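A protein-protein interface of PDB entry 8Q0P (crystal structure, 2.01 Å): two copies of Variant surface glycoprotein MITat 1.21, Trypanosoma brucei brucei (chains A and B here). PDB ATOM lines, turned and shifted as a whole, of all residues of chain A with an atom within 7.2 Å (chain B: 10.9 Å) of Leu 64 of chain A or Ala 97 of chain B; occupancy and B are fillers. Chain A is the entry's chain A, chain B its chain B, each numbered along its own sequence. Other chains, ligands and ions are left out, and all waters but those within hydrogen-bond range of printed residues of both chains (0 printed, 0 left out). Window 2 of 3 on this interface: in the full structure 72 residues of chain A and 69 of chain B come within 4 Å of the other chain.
CE of Lys 104 of chain B touches CA of Lys 58 of chain A, at 3.7 Å.
Ile 100 of chain B touches Gln 61 of chain A.
Leu 64 of chain A touches Ala 97 of chain B.
CG2 of Ile 100 of chain A touches OE1 of Gln 61 of chain B, 3.4 Å away.
Ile 100 of chain A touches Ile 100 of chain B (CD1 to CD1, 3.5 Å).
NZ of Lys 104 of chain B is in hydrogen-bond range of OE1 of Gln 61 of chain A (3.1 Å).
O of Ala 97 of chain A sits close to OE1 of Gln 61 of chain B, at 3.4 Å.
The side-chain amide nitrogen of Gln 61 of chain A lies within hydrogen-bond range of the side-chain carboxylate of Glu 101 of chain B.
Printed residues of chain B that touch a printed residue of chain A: Gln 61, Ala 97, Ile 100, Glu 101 and Lys 104.
Hydrophobic or aromatic side chains of chain B that line the printed part of chain A: Ile 100.
Along chain B the printed residues that touch a printed residue of chain A span positions 61 to 104.
Hydrophobic or aromatic side chains of chain A that line the printed part of chain B: Leu 64 and Ile 100.
Gln 61 of chain A touches Ile 100 of chain B, and with the chains exchanged Ile 100 of chain A touches Gln 61 of chain B.
Ala 97 of chain A touches Gln 61 of chain B, but with the chains exchanged Gln 61 of chain A does not touch Ala 97 of chain B (5.4 Å).
Ile 100 of chain A touches its own counterpart, Ile 100 of chain B.
Of the 8 pairs that touch across the chains among the printed residues, 3 have their exchanged pair printed and touching as well.
Of the printed residues of chain B, Gln 61 of chain A touches Ile 100, Glu 101 and Lys 104.
No residue of chain B comes within 4 Å of Ala 63 of chain A.
Of chain B, only Ala 97 (3.9 Å) comes within 4 Å of Leu 64 of chain A.
No residue of chain B comes within 4 Å of Ala 96 of chain A.
Of the printed residues of chain B, Ala 97 of chain A touches Gln 61.
Ser 94 of chain B touches none of the printed residues of chain A.
No residue of chain A comes within 4 Å of Ala 96 of chain B.
Ala 97 of chain B touches just one residue of chain A: Leu 64 (3.9 Å).
Of the printed residues of chain A, Ile 100 of chain B touches Gln 61 (3.8 Å) and Ile 100 (3.5 Å).
Printed residues of chain A within 4 Å of Glu 101 of chain B: Gln 61.
The nearest printed residue of chain A that does not touch Ile 100 of chain B is Leu 64 of chain A (4.2 Å).
O of Glu 101 of chain B lies within hydrogen-bond range of OG1 of Thr 105 of chain B (3.1 Å).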
ATOM      1  N   LYS A  58     -21.600 -14.181  16.472  1.00  0.00           N
ATOM      2  CA  LYS A  58     -21.356 -14.212  15.035  1.00  0.00           C
ATOM      3  C   LYS A  58     -21.819 -12.923  14.370  1.00  0.00           C
ATOM      4  O   LYS A  58     -21.178 -12.437  13.430  1.00  0.00           O
ATOM      5  CB  LYS A  58     -22.053 -15.421  14.411  1.00  0.00           C
ATOM      6  CG  LYS A  58     -21.688 -15.671  12.951  1.00  0.00           C
ATOM      7  CD  LYS A  58     -22.815 -16.391  12.224  1.00  0.00           C
ATOM      8  CE  LYS A  58     -22.470 -16.659  10.772  1.00  0.00           C
ATOM      9  NZ  LYS A  58     -20.998 -16.653  10.523  1.00  0.00           N
ATOM     10  N   THR A  59     -22.931 -12.356  14.840  1.00  0.00           N
ATOM     11  CA  THR A  59     -23.399 -11.091  14.285  1.00  0.00           C
ATOM     12  C   THR A  59     -22.388  -9.982  14.534  1.00  0.00           C
ATOM     13  O   THR A  59     -22.081  -9.197  13.630  1.00  0.00           O
ATOM     14  CB  THR A  59     -24.763 -10.734  14.875  1.00  0.00           C
ATOM     15  OG1 THR A  59     -25.777 -11.520  14.235  1.00  0.00           O
ATOM     16  CG2 THR A  59     -25.072  -9.266  14.665  1.00  0.00           C
ATOM     17  N   ALA A  60     -21.839  -9.916  15.749  1.00  0.00           N
ATOM     18  CA  ALA A  60     -20.786  -8.942  16.017  1.00  0.00           C
ATOM     19  C   ALA A  60     -19.528  -9.241  15.212  1.00  0.00           C
ATOM     20  O   ALA A  60     -18.842  -8.313  14.770  1.00  0.00           O
ATOM     21  CB  ALA A  60     -20.467  -8.903  17.510  1.00  0.00           C
ATOM     22  N   GLN A  61     -19.218 -10.522  15.005  1.00  0.00           N
ATOM     23  CA  GLN A  61     -18.039 -10.889  14.227  1.00  0.00           C
ATOM     24  C   GLN A  61     -18.203 -10.514  12.758  1.00  0.00           C
ATOM     25  O   GLN A  61     -17.246 -10.064  12.116  1.00  0.00           O
ATOM     26  CB  GLN A  61     -17.767 -12.384  14.375  1.00  0.00           C
ATOM     27  CG  GLN A  61     -16.327 -12.790  14.130  1.00  0.00           C
ATOM     28  CD  GLN A  61     -16.200 -14.266  13.803  1.00  0.00           C
ATOM     29  OE1 GLN A  61     -17.025 -14.824  13.078  1.00  0.00           O
ATOM     30  NE2 GLN A  61     -15.173 -14.910  14.350  1.00  0.00           N
ATOM     31  N   SER A  62     -19.409 -10.695  12.207  1.00  0.00           N
ATOM     32  CA  SER A  62     -19.636 -10.351  10.807  1.00  0.00           C
ATOM     33  C   SER A  62     -19.556  -8.847  10.578  1.00  0.00           C
ATOM     34  O   SER A  62     -19.209  -8.407   9.476  1.00  0.00           O
ATOM     35  CB  SER A  62     -20.988 -10.891  10.344  1.00  0.00           C
ATOM     36  OG  SER A  62     -22.049 -10.058  10.781  1.00  0.00           O
ATOM     37  N   ALA A  63     -19.861  -8.049  11.601  1.00  0.00           N
ATOM     38  CA  ALA A  63     -19.791  -6.597  11.531  1.00  0.00           C
ATOM     39  C   ALA A  63     -18.373  -6.063  11.693  1.00  0.00           C
ATOM     40  O   ALA A  63     -18.204  -4.884  12.023  1.00  0.00           O
ATOM     41  CB  ALA A  63     -20.707  -5.977  12.590  1.00  0.00           C
ATOM     42  N   LEU A  64     -17.355  -6.888  11.468  1.00  0.00           N
ATOM     43  CA  LEU A  64     -15.973  -6.443  11.595  1.00  0.00           C
ATOM     44  C   LEU A  64     -15.187  -6.721  10.319  1.00  0.00           C
ATOM     45  O   LEU A  64     -15.721  -7.272   9.358  1.00  0.00           O
ATOM     46  CB  LEU A  64     -15.304  -7.122  12.788  1.00  0.00           C
ATOM     47  CG  LEU A  64     -15.746  -6.658  14.180  1.00  0.00           C
ATOM     48  CD1 LEU A  64     -15.057  -7.489  15.248  1.00  0.00           C
ATOM     49  CD2 LEU A  64     -15.457  -5.180  14.387  1.00  0.00           C
ATOM     50  N   SER A  94     -20.247   2.234  15.241  1.00  0.00           N
ATOM     51  CA  SER A  94     -20.331   1.002  14.463  1.00  0.00           C
ATOM     52  C   SER A  94     -21.312   0.030  15.105  1.00  0.00           C
ATOM     53  O   SER A  94     -21.509   0.051  16.320  1.00  0.00           O
ATOM     54  CB  SER A  94     -18.954   0.348  14.337  1.00  0.00           C
ATOM     55  OG  SER A  94     -18.315   0.258  15.600  1.00  0.00           O
ATOM     56  N   ALA A  96     -20.898  -3.151  15.418  1.00  0.00           N
ATOM     57  CA  ALA A  96     -20.178  -4.097  16.264  1.00  0.00           C
ATOM     58  C   ALA A  96     -19.987  -3.549  17.673  1.00  0.00           C
ATOM     59  O   ALA A  96     -19.890  -4.324  18.634  1.00  0.00           O
ATOM     60  CB  ALA A  96     -18.829  -4.445  15.638  1.00  0.00           C
ATOM     61  N   ALA A  97     -19.984  -2.232  17.831  1.00  0.00           N
ATOM     62  CA  ALA A  97     -19.728  -1.720  19.193  1.00  0.00           C
ATOM     63  C   ALA A  97     -20.967  -1.953  20.055  1.00  0.00           C
ATOM     64  O   ALA A  97     -20.811  -2.282  21.235  1.00  0.00           O
ATOM     65  CB  ALA A  97     -19.378  -0.259  19.148  1.00  0.00           C
ATOM     66  N   ILE A 100     -21.380  -5.929  20.887  1.00  0.00           N
ATOM     67  CA  ILE A 100     -20.530  -6.272  22.024  1.00  0.00           C
ATOM     68  C   ILE A 100     -21.081  -5.659  23.307  1.00  0.00           C
ATOM     69  O   ILE A 100     -21.070  -6.296  24.369  1.00  0.00           O
ATOM     70  CB  ILE A 100     -19.082  -5.820  21.757  1.00  0.00           C
ATOM     71  CG1 ILE A 100     -18.468  -6.603  20.593  1.00  0.00           C
ATOM     72  CG2 ILE A 100     -18.228  -5.991  23.003  1.00  0.00           C
ATOM     73  CD1 ILE A 100     -18.762  -8.085  20.627  1.00  0.00           C
ATOM     74  N   GLY B  56     -12.733 -10.655  29.142  1.00  0.00           N
ATOM     75  CA  GLY B  56     -12.537 -10.856  27.719  1.00  0.00           C
ATOM     76  C   GLY B  56     -13.445  -9.989  26.871  1.00  0.00           C
ATOM     77  O   GLY B  56     -13.058  -9.550  25.784  1.00  0.00           O
ATOM     78  N   LEU B  57     -14.659  -9.725  27.354  1.00  0.00           N
ATOM     79  CA  LEU B  57     -15.567  -8.830  26.656  1.00  0.00           C
ATOM     80  C   LEU B  57     -15.163  -7.373  26.838  1.00  0.00           C
ATOM     81  O   LEU B  57     -15.320  -6.573  25.910  1.00  0.00           O
ATOM     82  CB  LEU B  57     -16.996  -9.063  27.146  1.00  0.00           C
ATOM     83  CG  LEU B  57     -17.637 -10.357  26.635  1.00  0.00           C
ATOM     84  CD1 LEU B  57     -18.958 -10.627  27.346  1.00  0.00           C
ATOM     85  CD2 LEU B  57     -17.839 -10.316  25.134  1.00  0.00           C
ATOM     86  N   THR B  59     -12.144  -6.230  27.122  1.00  0.00           N
ATOM     87  CA  THR B  59     -11.007  -6.026  26.198  1.00  0.00           C
ATOM     88  C   THR B  59     -11.576  -5.824  24.798  1.00  0.00           C
ATOM     89  O   THR B  59     -11.149  -4.889  24.123  1.00  0.00           O
ATOM     90  CB  THR B  59     -10.035  -7.205  26.284  1.00  0.00           C
ATOM     91  OG1 THR B  59      -9.480  -7.208  27.599  1.00  0.00           O
ATOM     92  CG2 THR B  59      -8.928  -7.141  25.254  1.00  0.00           C
ATOM     93  N   ALA B  60     -12.523  -6.667  24.399  1.00  0.00           N
ATOM     94  CA  ALA B  60     -13.086  -6.568  23.036  1.00  0.00           C
ATOM     95  C   ALA B  60     -13.790  -5.217  22.873  1.00  0.00           C
ATOM     96  O   ALA B  60     -13.642  -4.600  21.810  1.00  0.00           O
ATOM     97  CB  ALA B  60     -14.012  -7.722  22.774  1.00  0.00           C
ATOM     98  N   GLN B  61     -14.506  -4.773  23.900  1.00  0.00           N
ATOM     99  CA  GLN B  61     -15.160  -3.446  23.844  1.00  0.00           C
ATOM    100  C   GLN B  61     -14.088  -2.440  23.431  1.00  0.00           C
ATOM    101  O   GLN B  61     -14.337  -1.677  22.483  1.00  0.00           O
ATOM    102  CB  GLN B  61     -15.775  -3.094  25.197  1.00  0.00           C
ATOM    103  CG  GLN B  61     -16.849  -2.024  25.119  1.00  0.00           C
ATOM    104  CD  GLN B  61     -18.230  -2.623  25.024  1.00  0.00           C
ATOM    105  OE1 GLN B  61     -18.781  -2.791  23.940  1.00  0.00           O
ATOM    106  NE2 GLN B  61     -18.800  -2.951  26.171  1.00  0.00           N
ATOM    107  N   SER B  62     -12.950  -2.432  24.125  1.00  0.00           N
ATOM    108  CA  SER B  62     -11.823  -1.568  23.701  1.00  0.00           C
ATOM    109  C   SER B  62     -11.494  -1.892  22.240  1.00  0.00           C
ATOM    110  O   SER B  62     -10.999  -3.005  22.006  1.00  0.00           O
ATOM    111  CB  SER B  62     -10.655  -1.750  24.623  1.00  0.00           C
ATOM    112  OG  SER B  62     -11.093  -1.775  25.973  1.00  0.00           O
ATOM    113  N   ALA B  63     -11.775  -0.972  21.310  1.00  0.00           N
ATOM    114  CA  ALA B  63     -11.619  -1.205  19.851  1.00  0.00           C
ATOM    115  C   ALA B  63     -12.785  -2.071  19.362  1.00  0.00           C
ATOM    116  O   ALA B  63     -13.919  -1.552  19.368  1.00  0.00           O
ATOM    117  CB  ALA B  63     -10.286  -1.806  19.489  1.00  0.00           C
ATOM    118  N   SER B  94      -8.487  -5.236  14.279  1.00  0.00           N
ATOM    119  CA  SER B  94      -8.090  -6.656  14.108  1.00  0.00           C
ATOM    120  C   SER B  94      -7.937  -7.256  15.504  1.00  0.00           C
ATOM    121  O   SER B  94      -8.219  -8.445  15.659  1.00  0.00           O
ATOM    122  CB  SER B  94      -6.825  -6.791  13.325  1.00  0.00           C
ATOM    123  OG  SER B  94      -6.403  -8.147  13.289  1.00  0.00           O
ATOM    124  N   GLU B  95      -7.493  -6.450  16.470  1.00  0.00           N
ATOM    125  CA  GLU B  95      -7.419  -6.932  17.870  1.00  0.00           C
ATOM    126  C   GLU B  95      -8.844  -7.198  18.346  1.00  0.00           C
ATOM    127  O   GLU B  95      -9.106  -8.301  18.837  1.00  0.00           O
ATOM    128  CB  GLU B  95      -6.778  -5.879  18.765  1.00  0.00           C
ATOM    129  CG  GLU B  95      -6.604  -6.336  20.200  1.00  0.00           C
ATOM    130  CD  GLU B  95      -6.007  -5.282  21.114  1.00  0.00           C
ATOM    131  OE1 GLU B  95      -6.119  -4.087  20.782  1.00  0.00           O
ATOM    132  OE2 GLU B  95      -5.429  -5.657  22.154  1.00  0.00           O
ATOM    133  N   ALA B  96      -9.727  -6.215  18.198  1.00  0.00           N
ATOM    134  CA  ALA B  96     -11.140  -6.445  18.548  1.00  0.00           C
ATOM    135  C   ALA B  96     -11.602  -7.728  17.858  1.00  0.00           C
ATOM    136  O   ALA B  96     -12.289  -8.530  18.503  1.00  0.00           O
ATOM    137  CB  ALA B  96     -11.956  -5.263  18.118  1.00  0.00           C
ATOM    138  N   ALA B  97     -11.203  -7.919  16.605  1.00  0.00           N
ATOM    139  CA  ALA B  97     -11.615  -9.117  15.847  1.00  0.00           C
ATOM    140  C   ALA B  97     -10.988 -10.372  16.458  1.00  0.00           C
ATOM    141  O   ALA B  97     -11.621 -11.437  16.385  1.00  0.00           O
ATOM    142  CB  ALA B  97     -11.207  -8.963  14.409  1.00  0.00           C
ATOM    143  N   LYS B  98      -9.777 -10.253  16.992  1.00  0.00           N
ATOM    144  CA  LYS B  98      -9.087 -11.437  17.555  1.00  0.00           C
ATOM    145  C   LYS B  98      -9.876 -11.920  18.770  1.00  0.00           C
ATOM    146  O   LYS B  98     -10.248 -13.099  18.799  1.00  0.00           O
ATOM    147  CB  LYS B  98      -7.667 -11.062  17.979  1.00  0.00           C
ATOM    148  CG  LYS B  98      -6.626 -11.062  16.870  1.00  0.00           C
ATOM    149  CD  LYS B  98      -5.398 -10.252  17.219  1.00  0.00           C
ATOM    150  CE  LYS B  98      -4.859  -9.451  16.051  1.00  0.00           C
ATOM    151  NZ  LYS B  98      -4.456  -8.086  16.461  1.00  0.00           N
ATOM    152  N   ALA B  99     -10.103 -11.029  19.733  1.00  0.00           N
ATOM    153  CA  ALA B  99     -10.886 -11.375  20.933  1.00  0.00           C
ATOM    154  C   ALA B  99     -12.191 -12.052  20.515  1.00  0.00           C
ATOM    155  O   ALA B  99     -12.458 -13.154  20.991  1.00  0.00           O
ATOM    156  CB  ALA B  99     -11.159 -10.128  21.721  1.00  0.00           C
ATOM    157  N   ILE B 100     -12.960 -11.412  19.647  1.00  0.00           N
ATOM    158  CA  ILE B 100     -14.287 -11.977  19.290  1.00  0.00           C
ATOM    159  C   ILE B 100     -14.067 -13.402  18.795  1.00  0.00           C
ATOM    160  O   ILE B 100     -14.787 -14.296  19.245  1.00  0.00           O
ATOM    161  CB  ILE B 100     -15.017 -11.094  18.264  1.00  0.00           C
ATOM    162  CG1 ILE B 100     -15.324  -9.714  18.843  1.00  0.00           C
ATOM    163  CG2 ILE B 100     -16.281 -11.774  17.766  1.00  0.00           C
ATOM    164  CD1 ILE B 100     -15.676  -9.746  20.306  1.00  0.00           C
ATOM    165  N   GLU B 101     -13.086 -13.599  17.925  1.00  0.00           N
ATOM    166  CA  GLU B 101     -12.876 -14.952  17.350  1.00  0.00           C
ATOM    167  C   GLU B 101     -12.635 -15.941  18.494  1.00  0.00           C
ATOM    168  O   GLU B 101     -13.222 -17.024  18.472  1.00  0.00           O
ATOM    169  CB  GLU B 101     -11.704 -14.941  16.373  1.00  0.00           C
ATOM    170  CG  GLU B 101     -11.471 -16.277  15.700  1.00  0.00           C
ATOM    171  CD  GLU B 101     -12.577 -16.702  14.752  1.00  0.00           C
ATOM    172  OE1 GLU B 101     -13.413 -17.533  15.154  1.00  0.00           O
ATOM    173  OE2 GLU B 101     -12.602 -16.196  13.614  1.00  0.00           O
ATOM    174  N   THR B 102     -11.791 -15.561  19.448  1.00  0.00           N
ATOM    175  CA  THR B 102     -11.512 -16.434  20.615  1.00  0.00           C
ATOM    176  C   THR B 102     -12.813 -16.662  21.387  1.00  0.00           C
ATOM    177  O   THR B 102     -13.278 -17.811  21.437  1.00  0.00           O
ATOM    178  CB  THR B 102     -10.441 -15.806  21.511  1.00  0.00           C
ATOM    179  OG1 THR B 102      -9.344 -15.422  20.682  1.00  0.00           O
ATOM    180  CG2 THR B 102      -9.961 -16.740  22.598  1.00  0.00           C
ATOM    181  N   ILE B 103     -13.342 -15.596  21.976  1.00  0.00           N
ATOM    182  CA  ILE B 103     -14.593 -15.686  22.775  1.00  0.00           C
ATOM    183  C   ILE B 103     -15.563 -16.636  22.080  1.00  0.00           C
ATOM    184  O   ILE B 103     -16.249 -17.384  22.785  1.00  0.00           O
ATOM    185  CB  ILE B 103     -15.177 -14.275  22.963  1.00  0.00           C
ATOM    186  CG1 ILE B 103     -14.268 -13.403  23.829  1.00  0.00           C
ATOM    187  CG2 ILE B 103     -16.592 -14.332  23.514  1.00  0.00           C
ATOM    188  CD1 ILE B 103     -14.582 -11.934  23.755  1.00  0.00           C
ATOM    189  N   LYS B 104     -15.567 -16.656  20.751  1.00  0.00           N
ATOM    190  CA  LYS B 104     -16.583 -17.474  20.044  1.00  0.00           C
ATOM    191  C   LYS B 104     -16.121 -18.926  19.963  1.00  0.00           C
ATOM    192  O   LYS B 104     -16.939 -19.807  20.229  1.00  0.00           O
ATOM    193  CB  LYS B 104     -16.856 -16.902  18.653  1.00  0.00           C
ATOM    194  CG  LYS B 104     -17.633 -17.816  17.717  1.00  0.00           C
ATOM    195  CD  LYS B 104     -18.837 -17.146  17.102  1.00  0.00           C
ATOM    196  CE  LYS B 104     -18.501 -16.439  15.807  1.00  0.00           C
ATOM    197  NZ  LYS B 104     -17.644 -17.276  14.935  1.00  0.00           N
ATOM    198  N   THR B 105     -14.863 -19.152  19.596  1.00  0.00           N
ATOM    199  CA  THR B 105     -14.367 -20.538  19.407  1.00  0.00           C
ATOM    200  C   THR B 105     -14.382 -21.275  20.745  1.00  0.00           C
ATOM    201  O   THR B 105     -14.507 -22.500  20.735  1.00  0.00           O
ATOM    202  CB  THR B 105     -12.956 -20.544  18.813  1.00  0.00           C
ATOM    203  OG1 THR B 105     -12.165 -19.656  19.601  1.00  0.00           O
ATOM    204  CG2 THR B 105     -12.928 -20.130  17.360  1.00  0.00           C
ATOM    205  N   ILE B 292      -6.426 -13.177  25.931  1.00  0.00           N
ATOM    206  CA  ILE B 292      -6.892 -11.982  25.246  1.00  0.00           C
ATOM    207  C   ILE B 292      -7.321 -10.933  26.267  1.00  0.00           C
ATOM    208  O   ILE B 292      -6.532 -10.534  27.128  1.00  0.00           O
ATOM    209  CB  ILE B 292      -8.023 -12.326  24.260  1.00  0.00           C
ATOM    210  CG1 ILE B 292      -9.180 -13.024  24.978  1.00  0.00           C
ATOM    211  CG2 ILE B 292      -7.499 -13.205  23.142  1.00  0.00           C
ATOM    212  CD1 ILE B 292     -10.354 -12.129  25.250  1.00  0.00           C
